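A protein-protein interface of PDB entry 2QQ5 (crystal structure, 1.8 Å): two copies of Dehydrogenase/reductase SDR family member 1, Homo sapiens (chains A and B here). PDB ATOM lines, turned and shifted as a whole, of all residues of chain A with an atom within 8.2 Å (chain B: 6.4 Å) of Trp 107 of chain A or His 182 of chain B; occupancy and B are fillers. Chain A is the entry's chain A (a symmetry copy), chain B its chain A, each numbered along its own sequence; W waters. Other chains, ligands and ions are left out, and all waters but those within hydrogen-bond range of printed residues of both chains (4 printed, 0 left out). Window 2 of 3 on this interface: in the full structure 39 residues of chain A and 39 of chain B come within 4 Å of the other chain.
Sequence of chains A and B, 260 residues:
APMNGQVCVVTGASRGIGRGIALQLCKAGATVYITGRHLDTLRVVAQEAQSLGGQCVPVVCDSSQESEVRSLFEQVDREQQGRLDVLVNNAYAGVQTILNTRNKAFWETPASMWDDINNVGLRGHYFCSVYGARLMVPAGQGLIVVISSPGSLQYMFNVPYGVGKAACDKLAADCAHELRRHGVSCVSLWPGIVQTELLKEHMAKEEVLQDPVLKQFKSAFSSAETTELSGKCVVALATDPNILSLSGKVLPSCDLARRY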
ATOM      1  N   LYS A 104     -10.176   5.990 -18.807  1.00  0.00           N
ATOM      2  CA  LYS A 104      -8.802   6.290 -18.381  1.00  0.00           C
ATOM      3  C   LYS A 104      -8.872   7.570 -17.587  1.00  0.00           C
ATOM      4  O   LYS A 104      -9.565   8.514 -17.994  1.00  0.00           O
ATOM      5  CB  LYS A 104      -7.853   6.462 -19.562  1.00  0.00           C
ATOM      6  CG  LYS A 104      -7.659   5.184 -20.401  1.00  0.00           C
ATOM      7  N   ALA A 105      -8.166   7.601 -16.466  1.00  0.00           N
ATOM      8  CA  ALA A 105      -8.225   8.738 -15.544  1.00  0.00           C
ATOM      9  C   ALA A 105      -7.369   9.869 -16.067  1.00  0.00           C
ATOM     10  O   ALA A 105      -6.492   9.658 -16.922  1.00  0.00           O
ATOM     11  CB  ALA A 105      -7.755   8.324 -14.134  1.00  0.00           C
ATOM     12  N   PHE A 106      -7.589  11.072 -15.534  1.00  0.00           N
ATOM     13  CA  PHE A 106      -6.917  12.264 -16.068  1.00  0.00           C
ATOM     14  C   PHE A 106      -5.384  12.195 -15.989  1.00  0.00           C
ATOM     15  O   PHE A 106      -4.684  12.808 -16.798  1.00  0.00           O
ATOM     16  CB  PHE A 106      -7.448  13.551 -15.415  1.00  0.00           C
ATOM     17  CG  PHE A 106      -6.946  13.802 -14.013  1.00  0.00           C
ATOM     18  CD1 PHE A 106      -5.773  14.513 -13.802  1.00  0.00           C
ATOM     19  CD2 PHE A 106      -7.680  13.372 -12.895  1.00  0.00           C
ATOM     20  CE1 PHE A 106      -5.319  14.753 -12.498  1.00  0.00           C
ATOM     21  CE2 PHE A 106      -7.244  13.630 -11.604  1.00  0.00           C
ATOM     22  CZ  PHE A 106      -6.063  14.296 -11.399  1.00  0.00           C
ATOM     23  N   TRP A 107      -4.852  11.472 -15.016  1.00  0.00           N
ATOM     24  CA  TRP A 107      -3.391  11.296 -14.931  1.00  0.00           C
ATOM     25  C   TRP A 107      -2.861  10.177 -15.836  1.00  0.00           C
ATOM     26  O   TRP A 107      -1.655  10.035 -16.005  1.00  0.00           O
ATOM     27  CB  TRP A 107      -2.942  11.073 -13.474  1.00  0.00           C
ATOM     28  CG  TRP A 107      -3.455   9.831 -12.884  1.00  0.00           C
ATOM     29  CD1 TRP A 107      -2.854   8.620 -12.892  1.00  0.00           C
ATOM     30  CD2 TRP A 107      -4.701   9.666 -12.203  1.00  0.00           C
ATOM     31  NE1 TRP A 107      -3.642   7.702 -12.263  1.00  0.00           N
ATOM     32  CE2 TRP A 107      -4.773   8.316 -11.802  1.00  0.00           C
ATOM     33  CE3 TRP A 107      -5.742  10.535 -11.861  1.00  0.00           C
ATOM     34  CZ2 TRP A 107      -5.871   7.787 -11.105  1.00  0.00           C
ATOM     35  CZ3 TRP A 107      -6.838  10.014 -11.156  1.00  0.00           C
ATOM     36  CH2 TRP A 107      -6.887   8.648 -10.790  1.00  0.00           C
ATOM     37  N   GLU A 108      -3.759   9.367 -16.377  1.00  0.00           N
ATOM     38  CA  GLU A 108      -3.387   8.258 -17.260  1.00  0.00           C
ATOM     39  C   GLU A 108      -3.296   8.739 -18.700  1.00  0.00           C
ATOM     40  O   GLU A 108      -2.457   8.276 -19.467  1.00  0.00           O
ATOM     41  CB  GLU A 108      -4.381   7.099 -17.118  1.00  0.00           C
ATOM     42  CG  GLU A 108      -4.233   6.419 -15.791  1.00  0.00           C
ATOM     43  CD  GLU A 108      -5.284   5.359 -15.477  1.00  0.00           C
ATOM     44  OE1 GLU A 108      -6.436   5.452 -15.934  1.00  0.00           O
ATOM     45  OE2 GLU A 108      -4.941   4.433 -14.718  1.00  0.00           O
ATOM     46  N   THR A 109      -4.164   9.658 -19.063  1.00  0.00           N
ATOM     47  CA  THR A 109      -4.156  10.262 -20.387  1.00  0.00           C
ATOM     48  C   THR A 109      -3.092  11.372 -20.468  1.00  0.00           C
ATOM     49  O   THR A 109      -2.638  11.881 -19.442  1.00  0.00           O
ATOM     50  CB  THR A 109      -5.556  10.822 -20.729  1.00  0.00           C
ATOM     51  OG1 THR A 109      -6.092  11.573 -19.620  1.00  0.00           O
ATOM     52  CG2 THR A 109      -6.519   9.663 -21.068  1.00  0.00           C
ATOM     53  N   PRO A 110      -2.677  11.750 -21.689  1.00  0.00           N
ATOM     54  CA  PRO A 110      -1.658  12.794 -21.810  1.00  0.00           C
ATOM     55  C   PRO A 110      -2.165  14.134 -21.259  1.00  0.00           C
ATOM     56  O   PRO A 110      -3.358  14.434 -21.328  1.00  0.00           O
ATOM     57  CB  PRO A 110      -1.446  12.909 -23.333  1.00  0.00           C
ATOM     58  CG  PRO A 110      -1.938  11.633 -23.883  1.00  0.00           C
ATOM     59  CD  PRO A 110      -3.102  11.262 -23.007  1.00  0.00           C
ATOM     60  N   ALA A 111      -1.247  14.929 -20.721  1.00  0.00           N
ATOM     61  CA  ALA A 111      -1.603  16.240 -20.209  1.00  0.00           C
ATOM     62  C   ALA A 111      -2.200  17.089 -21.326  1.00  0.00           C
ATOM     63  O   ALA A 111      -3.131  17.861 -21.099  1.00  0.00           O
ATOM     64  CB  ALA A 111      -0.355  16.917 -19.559  1.00  0.00           C
ATOM     65  N   MET A 113      -4.209  16.387 -23.544  1.00  0.00           N
ATOM     66  CA  MET A 113      -5.622  16.122 -23.815  1.00  0.00           C
ATOM     67  C   MET A 113      -6.506  17.345 -23.509  1.00  0.00           C
ATOM     68  O   MET A 113      -7.543  17.543 -24.139  1.00  0.00           O
ATOM     69  CB  MET A 113      -6.131  14.874 -23.059  1.00  0.00           C
ATOM     70  CG  MET A 113      -7.520  14.415 -23.523  1.00  0.00           C
ATOM     71  SD  MET A 113      -8.115  12.926 -22.679  1.00  0.00           S
ATOM     72  CE  MET A 113      -8.275  13.489 -21.006  1.00  0.00           C
ATOM     73  N   VAL A 159     -12.313  14.553 -16.995  1.00  0.00           N
ATOM     74  CA  VAL A 159     -12.078  15.818 -16.334  1.00  0.00           C
ATOM     75  C   VAL A 159     -12.148  17.002 -17.294  1.00  0.00           C
ATOM     76  O   VAL A 159     -12.905  17.952 -17.058  1.00  0.00           O
ATOM     77  CB  VAL A 159     -10.801  15.807 -15.490  1.00  0.00           C
ATOM     78  CG1 VAL A 159     -10.511  17.199 -14.912  1.00  0.00           C
ATOM     79  CG2 VAL A 159     -10.941  14.751 -14.364  1.00  0.00           C
ATOM     80  N   PRO A 160     -11.334  16.984 -18.348  1.00  0.00           N
ATOM     81  CA  PRO A 160     -11.387  18.171 -19.210  1.00  0.00           C
ATOM     82  C   PRO A 160     -12.755  18.432 -19.826  1.00  0.00           C
ATOM     83  O   PRO A 160     -13.112  19.595 -20.019  1.00  0.00           O
ATOM     84  CB  PRO A 160     -10.365  17.872 -20.297  1.00  0.00           C
ATOM     85  CG  PRO A 160      -9.470  16.867 -19.722  1.00  0.00           C
ATOM     86  CD  PRO A 160     -10.308  16.022 -18.798  1.00  0.00           C
ATOM     87  N   TYR B 126      -4.256  22.444 -14.969  1.00  0.00           N
ATOM     88  CA  TYR B 126      -4.530  21.085 -15.474  1.00  0.00           C
ATOM     89  C   TYR B 126      -3.227  20.313 -15.691  1.00  0.00           C
ATOM     90  O   TYR B 126      -3.070  19.181 -15.232  1.00  0.00           O
ATOM     91  CB  TYR B 126      -5.383  21.068 -16.757  1.00  0.00           C
ATOM     92  CG  TYR B 126      -5.766  19.655 -17.175  1.00  0.00           C
ATOM     93  CD1 TYR B 126      -6.794  18.984 -16.524  1.00  0.00           C
ATOM     94  CD2 TYR B 126      -5.068  18.973 -18.178  1.00  0.00           C
ATOM     95  CE1 TYR B 126      -7.150  17.717 -16.872  1.00  0.00           C
ATOM     96  CE2 TYR B 126      -5.419  17.663 -18.537  1.00  0.00           C
ATOM     97  CZ  TYR B 126      -6.457  17.050 -17.877  1.00  0.00           C
ATOM     98  OH  TYR B 126      -6.878  15.789 -18.191  1.00  0.00           O
ATOM     99  N   SER B 129      -1.696  19.372 -12.396  1.00  0.00           N
ATOM    100  CA  SER B 129      -2.474  18.336 -11.749  1.00  0.00           C
ATOM    101  C   SER B 129      -2.207  16.955 -12.343  1.00  0.00           C
ATOM    102  O   SER B 129      -2.112  15.986 -11.608  1.00  0.00           O
ATOM    103  CB  SER B 129      -3.957  18.666 -11.790  1.00  0.00           C
ATOM    104  OG  SER B 129      -4.209  19.825 -11.003  1.00  0.00           O
ATOM    105  N   VAL B 130      -2.105  16.875 -13.660  1.00  0.00           N
ATOM    106  CA  VAL B 130      -1.798  15.608 -14.331  1.00  0.00           C
ATOM    107  C   VAL B 130      -0.471  15.036 -13.820  1.00  0.00           C
ATOM    108  O   VAL B 130      -0.417  13.887 -13.331  1.00  0.00           O
ATOM    109  CB  VAL B 130      -1.787  15.763 -15.892  1.00  0.00           C
ATOM    110  CG1 VAL B 130      -1.207  14.513 -16.568  1.00  0.00           C
ATOM    111  CG2 VAL B 130      -3.222  16.066 -16.417  1.00  0.00           C
ATOM    112  N   TYR B 131       0.598  15.837 -13.924  1.00  0.00           N
ATOM    113  CA  TYR B 131       1.938  15.362 -13.567  1.00  0.00           C
ATOM    114  C   TYR B 131       2.106  15.088 -12.072  1.00  0.00           C
ATOM    115  O   TYR B 131       2.749  14.117 -11.684  1.00  0.00           O
ATOM    116  CB  TYR B 131       3.027  16.304 -14.129  1.00  0.00           C
ATOM    117  CG  TYR B 131       3.143  16.167 -15.634  1.00  0.00           C
ATOM    118  CD1 TYR B 131       3.712  15.044 -16.207  1.00  0.00           C
ATOM    119  CD2 TYR B 131       2.651  17.157 -16.494  1.00  0.00           C
ATOM    120  CE1 TYR B 131       3.807  14.901 -17.599  1.00  0.00           C
ATOM    121  CE2 TYR B 131       2.750  17.029 -17.878  1.00  0.00           C
ATOM    122  CZ  TYR B 131       3.313  15.903 -18.427  1.00  0.00           C
ATOM    123  OH  TYR B 131       3.415  15.774 -19.796  1.00  0.00           O
ATOM    124  N   ALA B 133      -0.510  14.319  -9.930  1.00  0.00           N
ATOM    125  CA  ALA B 133      -1.332  13.149  -9.644  1.00  0.00           C
ATOM    126  C   ALA B 133      -0.559  11.867 -10.000  1.00  0.00           C
ATOM    127  O   ALA B 133      -0.679  10.833  -9.316  1.00  0.00           O
ATOM    128  CB  ALA B 133      -2.667  13.229 -10.402  1.00  0.00           C
ATOM    129  N   ARG B 134       0.215  11.903 -11.086  1.00  0.00           N
ATOM    130  CA  ARG B 134       1.030  10.732 -11.461  1.00  0.00           C
ATOM    131  C   ARG B 134       1.963  10.298 -10.329  1.00  0.00           C
ATOM    132  O   ARG B 134       2.180   9.105 -10.127  1.00  0.00           O
ATOM    133  CB  ARG B 134       1.836  10.958 -12.741  1.00  0.00           C
ATOM    134  CG  ARG B 134       0.966  10.891 -13.956  1.00  0.00           C
ATOM    135  CD  ARG B 134       1.713  11.282 -15.208  1.00  0.00           C
ATOM    136  NE  ARG B 134       0.767  11.305 -16.315  1.00  0.00           N
ATOM    137  CZ  ARG B 134       1.107  11.513 -17.578  1.00  0.00           C
ATOM    138  NH1 ARG B 134       2.378  11.711 -17.911  1.00  0.00           N
ATOM    139  NH2 ARG B 134       0.166  11.504 -18.505  1.00  0.00           N
ATOM    140  N   MET B 136       1.363  11.149  -6.983  1.00  0.00           N
ATOM    141  CA  MET B 136       0.570  10.882  -5.776  1.00  0.00           C
ATOM    142  C   MET B 136      -0.115   9.508  -5.805  1.00  0.00           C
ATOM    143  O   MET B 136      -0.149   8.801  -4.794  1.00  0.00           O
ATOM    144  CB  MET B 136      -0.479  11.962  -5.590  1.00  0.00           C
ATOM    145  CG  MET B 136       0.119  13.328  -5.386  1.00  0.00           C
ATOM    146  SD  MET B 136      -1.144  14.538  -5.066  1.00  0.00           S
ATOM    147  CE  MET B 136      -0.129  16.014  -4.795  1.00  0.00           C
ATOM    148  N   VAL B 137      -0.730   9.174  -6.949  1.00  0.00           N
ATOM    149  CA  VAL B 137      -1.624   8.024  -7.014  1.00  0.00           C
ATOM    150  C   VAL B 137      -0.947   6.714  -6.548  1.00  0.00           C
ATOM    151  O   VAL B 137      -1.534   5.993  -5.742  1.00  0.00           O
ATOM    152  CB  VAL B 137      -2.340   7.922  -8.383  1.00  0.00           C
ATOM    153  CG1 VAL B 137      -3.057   6.599  -8.565  1.00  0.00           C
ATOM    154  CG2 VAL B 137      -3.333   9.128  -8.540  1.00  0.00           C
ATOM    155  N   PRO B 138       0.297   6.426  -7.000  1.00  0.00           N
ATOM    156  CA  PRO B 138       1.057   5.240  -6.549  1.00  0.00           C
ATOM    157  C   PRO B 138       1.260   5.163  -5.035  1.00  0.00           C
ATOM    158  O   PRO B 138       1.326   4.073  -4.494  1.00  0.00           O
ATOM    159  CB  PRO B 138       2.406   5.404  -7.265  1.00  0.00           C
ATOM    160  CG  PRO B 138       2.109   6.165  -8.451  1.00  0.00           C
ATOM    161  CD  PRO B 138       1.052   7.158  -8.037  1.00  0.00           C
ATOM    162  N   ALA B 139       1.324   6.314  -4.364  1.00  0.00           N
ATOM    163  CA  ALA B 139       1.505   6.387  -2.905  1.00  0.00           C
ATOM    164  C   ALA B 139       0.199   6.219  -2.093  1.00  0.00           C
ATOM    165  O   ALA B 139       0.232   6.037  -0.881  1.00  0.00           O
ATOM    166  CB  ALA B 139       2.196   7.702  -2.536  1.00  0.00           C
ATOM    167  N   GLY B 140      -0.942   6.284  -2.762  1.00  0.00           N
ATOM    168  CA  GLY B 140      -2.247   6.183  -2.102  1.00  0.00           C
ATOM    169  C   GLY B 140      -2.621   7.313  -1.164  1.00  0.00           C
ATOM    170  O   GLY B 140      -3.445   7.144  -0.252  1.00  0.00           O
ATOM    171  N   GLN B 141      -2.010   8.474  -1.376  1.00  0.00           N
ATOM    172  CA  GLN B 141      -2.228   9.634  -0.536  1.00  0.00           C
ATOM    173  C   GLN B 141      -1.693  10.887  -1.249  1.00  0.00           C
ATOM    174  O   GLN B 141      -0.912  10.807  -2.239  1.00  0.00           O
ATOM    175  CB  GLN B 141      -1.558   9.450   0.838  1.00  0.00           C
ATOM    176  CG  GLN B 141      -0.056   9.382   0.751  1.00  0.00           C
ATOM    177  CD  GLN B 141       0.620   8.882   2.023  1.00  0.00           C
ATOM    178  OE1 GLN B 141       0.045   8.113   2.798  1.00  0.00           O
ATOM    179  NE2 GLN B 141       1.873   9.299   2.221  1.00  0.00           N
ATOM    180  N   CYS B 175     -11.419  16.220 -10.521  1.00  0.00           N
ATOM    181  CA  CYS B 175     -10.192  15.516 -10.127  1.00  0.00           C
ATOM    182  C   CYS B 175     -10.405  14.725  -8.835  1.00  0.00           C
ATOM    183  O   CYS B 175      -9.979  13.564  -8.736  1.00  0.00           O
ATOM    184  CB  CYS B 175      -9.021  16.495  -9.949  1.00  0.00           C
ATOM    185  SG  CYS B 175      -8.409  17.147 -11.508  1.00  0.00           S
ATOM    186  N   GLU B 178     -12.229  11.369  -9.453  1.00  0.00           N
ATOM    187  CA  GLU B 178     -11.397  10.284  -9.981  1.00  0.00           C
ATOM    188  C   GLU B 178     -10.353   9.818  -8.973  1.00  0.00           C
ATOM    189  O   GLU B 178      -9.967   8.644  -8.977  1.00  0.00           O
ATOM    190  CB  GLU B 178     -10.707  10.716 -11.274  1.00  0.00           C
ATOM    191  CG  GLU B 178     -11.692  10.955 -12.459  1.00  0.00           C
ATOM    192  CD  GLU B 178     -10.977  11.078 -13.817  1.00  0.00           C
ATOM    193  OE1 GLU B 178      -9.714  11.142 -13.824  1.00  0.00           O
ATOM    194  OE2 GLU B 178     -11.671  11.120 -14.858  1.00  0.00           O
ATOM    195  N   LEU B 179      -9.883  10.734  -8.126  1.00  0.00           N
ATOM    196  CA  LEU B 179      -8.791  10.426  -7.194  1.00  0.00           C
ATOM    197  C   LEU B 179      -9.211   9.721  -5.924  1.00  0.00           C
ATOM    198  O   LEU B 179      -8.389   9.094  -5.255  1.00  0.00           O
ATOM    199  CB  LEU B 179      -8.091  11.701  -6.790  1.00  0.00           C
ATOM    200  CG  LEU B 179      -7.235  12.289  -7.900  1.00  0.00           C
ATOM    201  CD1 LEU B 179      -6.892  13.735  -7.505  1.00  0.00           C
ATOM    202  CD2 LEU B 179      -5.987  11.425  -8.168  1.00  0.00           C
ATOM    203  N   ARG B 180     -10.479   9.828  -5.585  1.00  0.00           N
ATOM    204  CA  ARG B 180     -10.937   9.382  -4.271  1.00  0.00           C
ATOM    205  C   ARG B 180     -10.607   7.917  -3.991  1.00  0.00           C
ATOM    206  O   ARG B 180     -10.172   7.564  -2.887  1.00  0.00           O
ATOM    207  CB  ARG B 180     -12.432   9.597  -4.154  1.00  0.00           C
ATOM    208  CG  ARG B 180     -12.980   9.276  -2.746  1.00  0.00           C
ATOM    209  CD  ARG B 180     -14.427   9.602  -2.658  1.00  0.00           C
ATOM    210  NE  ARG B 180     -14.682  11.006  -2.916  1.00  0.00           N
ATOM    211  CZ  ARG B 180     -14.467  11.974  -2.034  1.00  0.00           C
ATOM    212  NH1 ARG B 180     -14.018  11.705  -0.801  1.00  0.00           N
ATOM    213  NH2 ARG B 180     -14.697  13.223  -2.382  1.00  0.00           N
ATOM    214  N   ARG B 181     -10.829   7.050  -4.978  1.00  0.00           N
ATOM    215  CA  ARG B 181     -10.601   5.621  -4.755  1.00  0.00           C
ATOM    216  C   ARG B 181      -9.129   5.284  -4.508  1.00  0.00           C
ATOM    217  O   ARG B 181      -8.822   4.209  -3.988  1.00  0.00           O
ATOM    218  CB  ARG B 181     -11.145   4.793  -5.923  1.00  0.00           C
ATOM    219  CG  ARG B 181     -10.327   4.908  -7.194  1.00  0.00           C
ATOM    220  CD  ARG B 181     -10.983   4.192  -8.352  1.00  0.00           C
ATOM    221  NE  ARG B 181     -11.202   2.779  -8.067  1.00  0.00           N
ATOM    222  CZ  ARG B 181     -10.349   1.794  -8.346  1.00  0.00           C
ATOM    223  NH1 ARG B 181      -9.174   2.043  -8.922  1.00  0.00           N
ATOM    224  NH2 ARG B 181     -10.680   0.539  -8.037  1.00  0.00           N
ATOM    225  N   HIS B 182      -8.236   6.199  -4.879  1.00  0.00           N
ATOM    226  CA  HIS B 182      -6.801   6.049  -4.683  1.00  0.00           C
ATOM    227  C   HIS B 182      -6.296   6.762  -3.425  1.00  0.00           C
ATOM    228  O   HIS B 182      -5.075   6.856  -3.177  1.00  0.00           O
ATOM    229  CB  HIS B 182      -6.066   6.615  -5.896  1.00  0.00           C
ATOM    230  CG  HIS B 182      -6.446   5.956  -7.181  1.00  0.00           C
ATOM    231  ND1 HIS B 182      -5.972   4.713  -7.541  1.00  0.00           N
ATOM    232  CD2 HIS B 182      -7.278   6.346  -8.178  1.00  0.00           C
ATOM    233  CE1 HIS B 182      -6.485   4.372  -8.710  1.00  0.00           C
ATOM    234  NE2 HIS B 182      -7.280   5.344  -9.119  1.00  0.00           N
ATOM    235  N   GLY B 183      -7.218   7.293  -2.638  1.00  0.00           N
ATOM    236  CA  GLY B 183      -6.850   7.950  -1.394  1.00  0.00           C
ATOM    237  C   GLY B 183      -6.250   9.341  -1.491  1.00  0.00           C
ATOM    238  O   GLY B 183      -5.758   9.866  -0.488  1.00  0.00           O
ATOM    239  N   VAL B 184      -6.315   9.947  -2.674  1.00  0.00           N
ATOM    240  CA  VAL B 184      -5.787  11.262  -2.893  1.00  0.00           C
ATOM    241  C   VAL B 184      -6.900  12.285  -2.906  1.00  0.00           C
ATOM    242  O   VAL B 184      -7.962  12.053  -3.471  1.00  0.00           O
ATOM    243  CB  VAL B 184      -4.991  11.323  -4.232  1.00  0.00           C
ATOM    244  CG1 VAL B 184      -4.447  12.727  -4.479  1.00  0.00           C
ATOM    245  CG2 VAL B 184      -3.850  10.258  -4.245  1.00  0.00           C
ATOM    246  N   LEU B 244      -9.533  13.439   3.353  1.00  0.00           N
ATOM    247  CA  LEU B 244     -10.341  12.859   2.275  1.00  0.00           C
ATOM    248  C   LEU B 244     -11.814  13.207   2.407  1.00  0.00           C
ATOM    249  O   LEU B 244     -12.519  13.302   1.405  1.00  0.00           O
ATOM    250  CB  LEU B 244     -10.136  11.339   2.206  1.00  0.00           C
ATOM    251  CG  LEU B 244     -10.333  10.573   0.891  1.00  0.00           C
ATOM    252  CD1 LEU B 244      -9.671  11.178  -0.338  1.00  0.00           C
ATOM    253  CD2 LEU B 244      -9.794   9.153   1.164  1.00  0.00           C
HETATM  254  O   HOH W   1      -0.314   9.460 -21.269  1.00  0.00           O
HETATM  255  O   HOH W   2       1.461  13.774 -20.598  1.00  0.00           O
HETATM  256  O   HOH W   3      -5.067  14.054 -19.292  1.00  0.00           O
HETATM  257  O   HOH W   4     -10.271  12.492 -16.880  1.00  0.00           O
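NE of Arg 134 of chain B sits at hydrogen-bond distance from O of Trp 107 of chain A (2.8 Å). O of Thr 109 of chain A sits at hydrogen-bond distance from NH2 of Arg 134 of chain B (3.0 Å). The side-chain carboxylate (OE1) of Glu 178 of chain B sits at hydrogen-bond distance from the backbone NH (N) of Phe 106 of chain A (2.7 Å).
The backbone NH (N) of Val 184 of chain B lies within hydrogen-bond range of the backbone carbonyl oxygen (O) of Leu 179 of chain B (3.4 Å). N of Ala 105 of chain A lies within hydrogen-bond range of OE1 of Glu 108 of chain A. The side-chain hydroxyl (OG1) of Thr 109 of chain A is in hydrogen-bond range of the backbone carbonyl oxygen (O) of Ala 105 of chain A. O of Phe 106 of chain A lies within hydrogen-bond range of OG1 of Thr 109 of chain A.
Glu 178 of chain B touches Ala 105 of chain A (OE1 to CA, 3.3 Å). Phe 106 of chain A touches Val 130 of chain B. Leu 179 of chain B touches Phe 106 of chain A. Val 137 of chain B touches Trp 107 of chain A. O of Glu 178 of chain B touches CH2 of Trp 107 of chain A, at 3.6 Å. Leu 179 of chain B touches Trp 107 of chain A (CD2 to CZ3, 3.4 Å). NH2 of Arg 134 of chain B touches CA of Pro 110 of chain A, 3.99 Å away. CG1 of Val 130 of chain B touches CB of Ala 111 of chain A, 3.9 Å away. Val 159 of chain A touches Tyr 126 of chain B (CG1 to CE1, 3.9 Å). Tyr 126 of chain B touches Pro 160 of chain A (OH to CG, 3.2 Å).
Trp 107 of chain A touches seven residues of chain B. Printed residues of chain B within 4 Å of Thr 109 of chain A: Arg 134 (3.0 Å). Printed residues of chain B within 4 Å of Ala 111 of chain A: Tyr 126, Val 130 and Tyr 131. Printed residues of chain A within 4 Å of Ala 133 of chain B: Phe 106 (3.7 Å) and Trp 107 (3.8 Å). Gly 140 of chain B touches none of the printed residues of chain A. The nearest printed residue of chain A that does not touch Ser 129 of chain B is Trp 107 of chain A (5.3 Å).
Printed residues of chain A that touch a printed residue of chain B: Ala 105, Phe 106, Trp 107, Thr 109, Pro 110, Ala 111, Met 113, Val 159 and Pro 160. Hydrophobic or aromatic side chains of chain A that line the printed part of chain B: Ala 105, Phe 106, Trp 107, Ala 111, Met 113, Val 159 and Pro 160. Among the printed residues, no Asp or Glu carboxylate lies within 4 Å of a Lys or Arg side-chain nitrogen of the other chain.
No position is printed for both chains.
Water W3 lies within hydrogen-bond range of the backbone carbonyl oxygen of Pro 110 of chain A (2.7 Å), the side-chain hydroxyl of Thr 109 of chain A (2.7 Å), the side-chain hydroxyl of Tyr 126 of chain B (2.7 Å) and the backbone carbonyl oxygen of Phe 106 of chain A (2.8 Å). Water W4 lies within hydrogen-bond range of OE2 of Glu 178 of chain B (2.8 Å), N of Val 159 of chain A (2.9 Å) and N of Phe 106 of chain A (3.3 Å). Water W2 lies within hydrogen-bond range of the side-chain hydroxyl (OH) of Tyr 131 of chain B, the backbone NH (N) of Ala 111 of chain A and the guanidinium group (NH2) of Arg 134 of chain B. Water W1 bridges O of Glu 108 of chain A and NH2 of Arg 134 of chain B.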
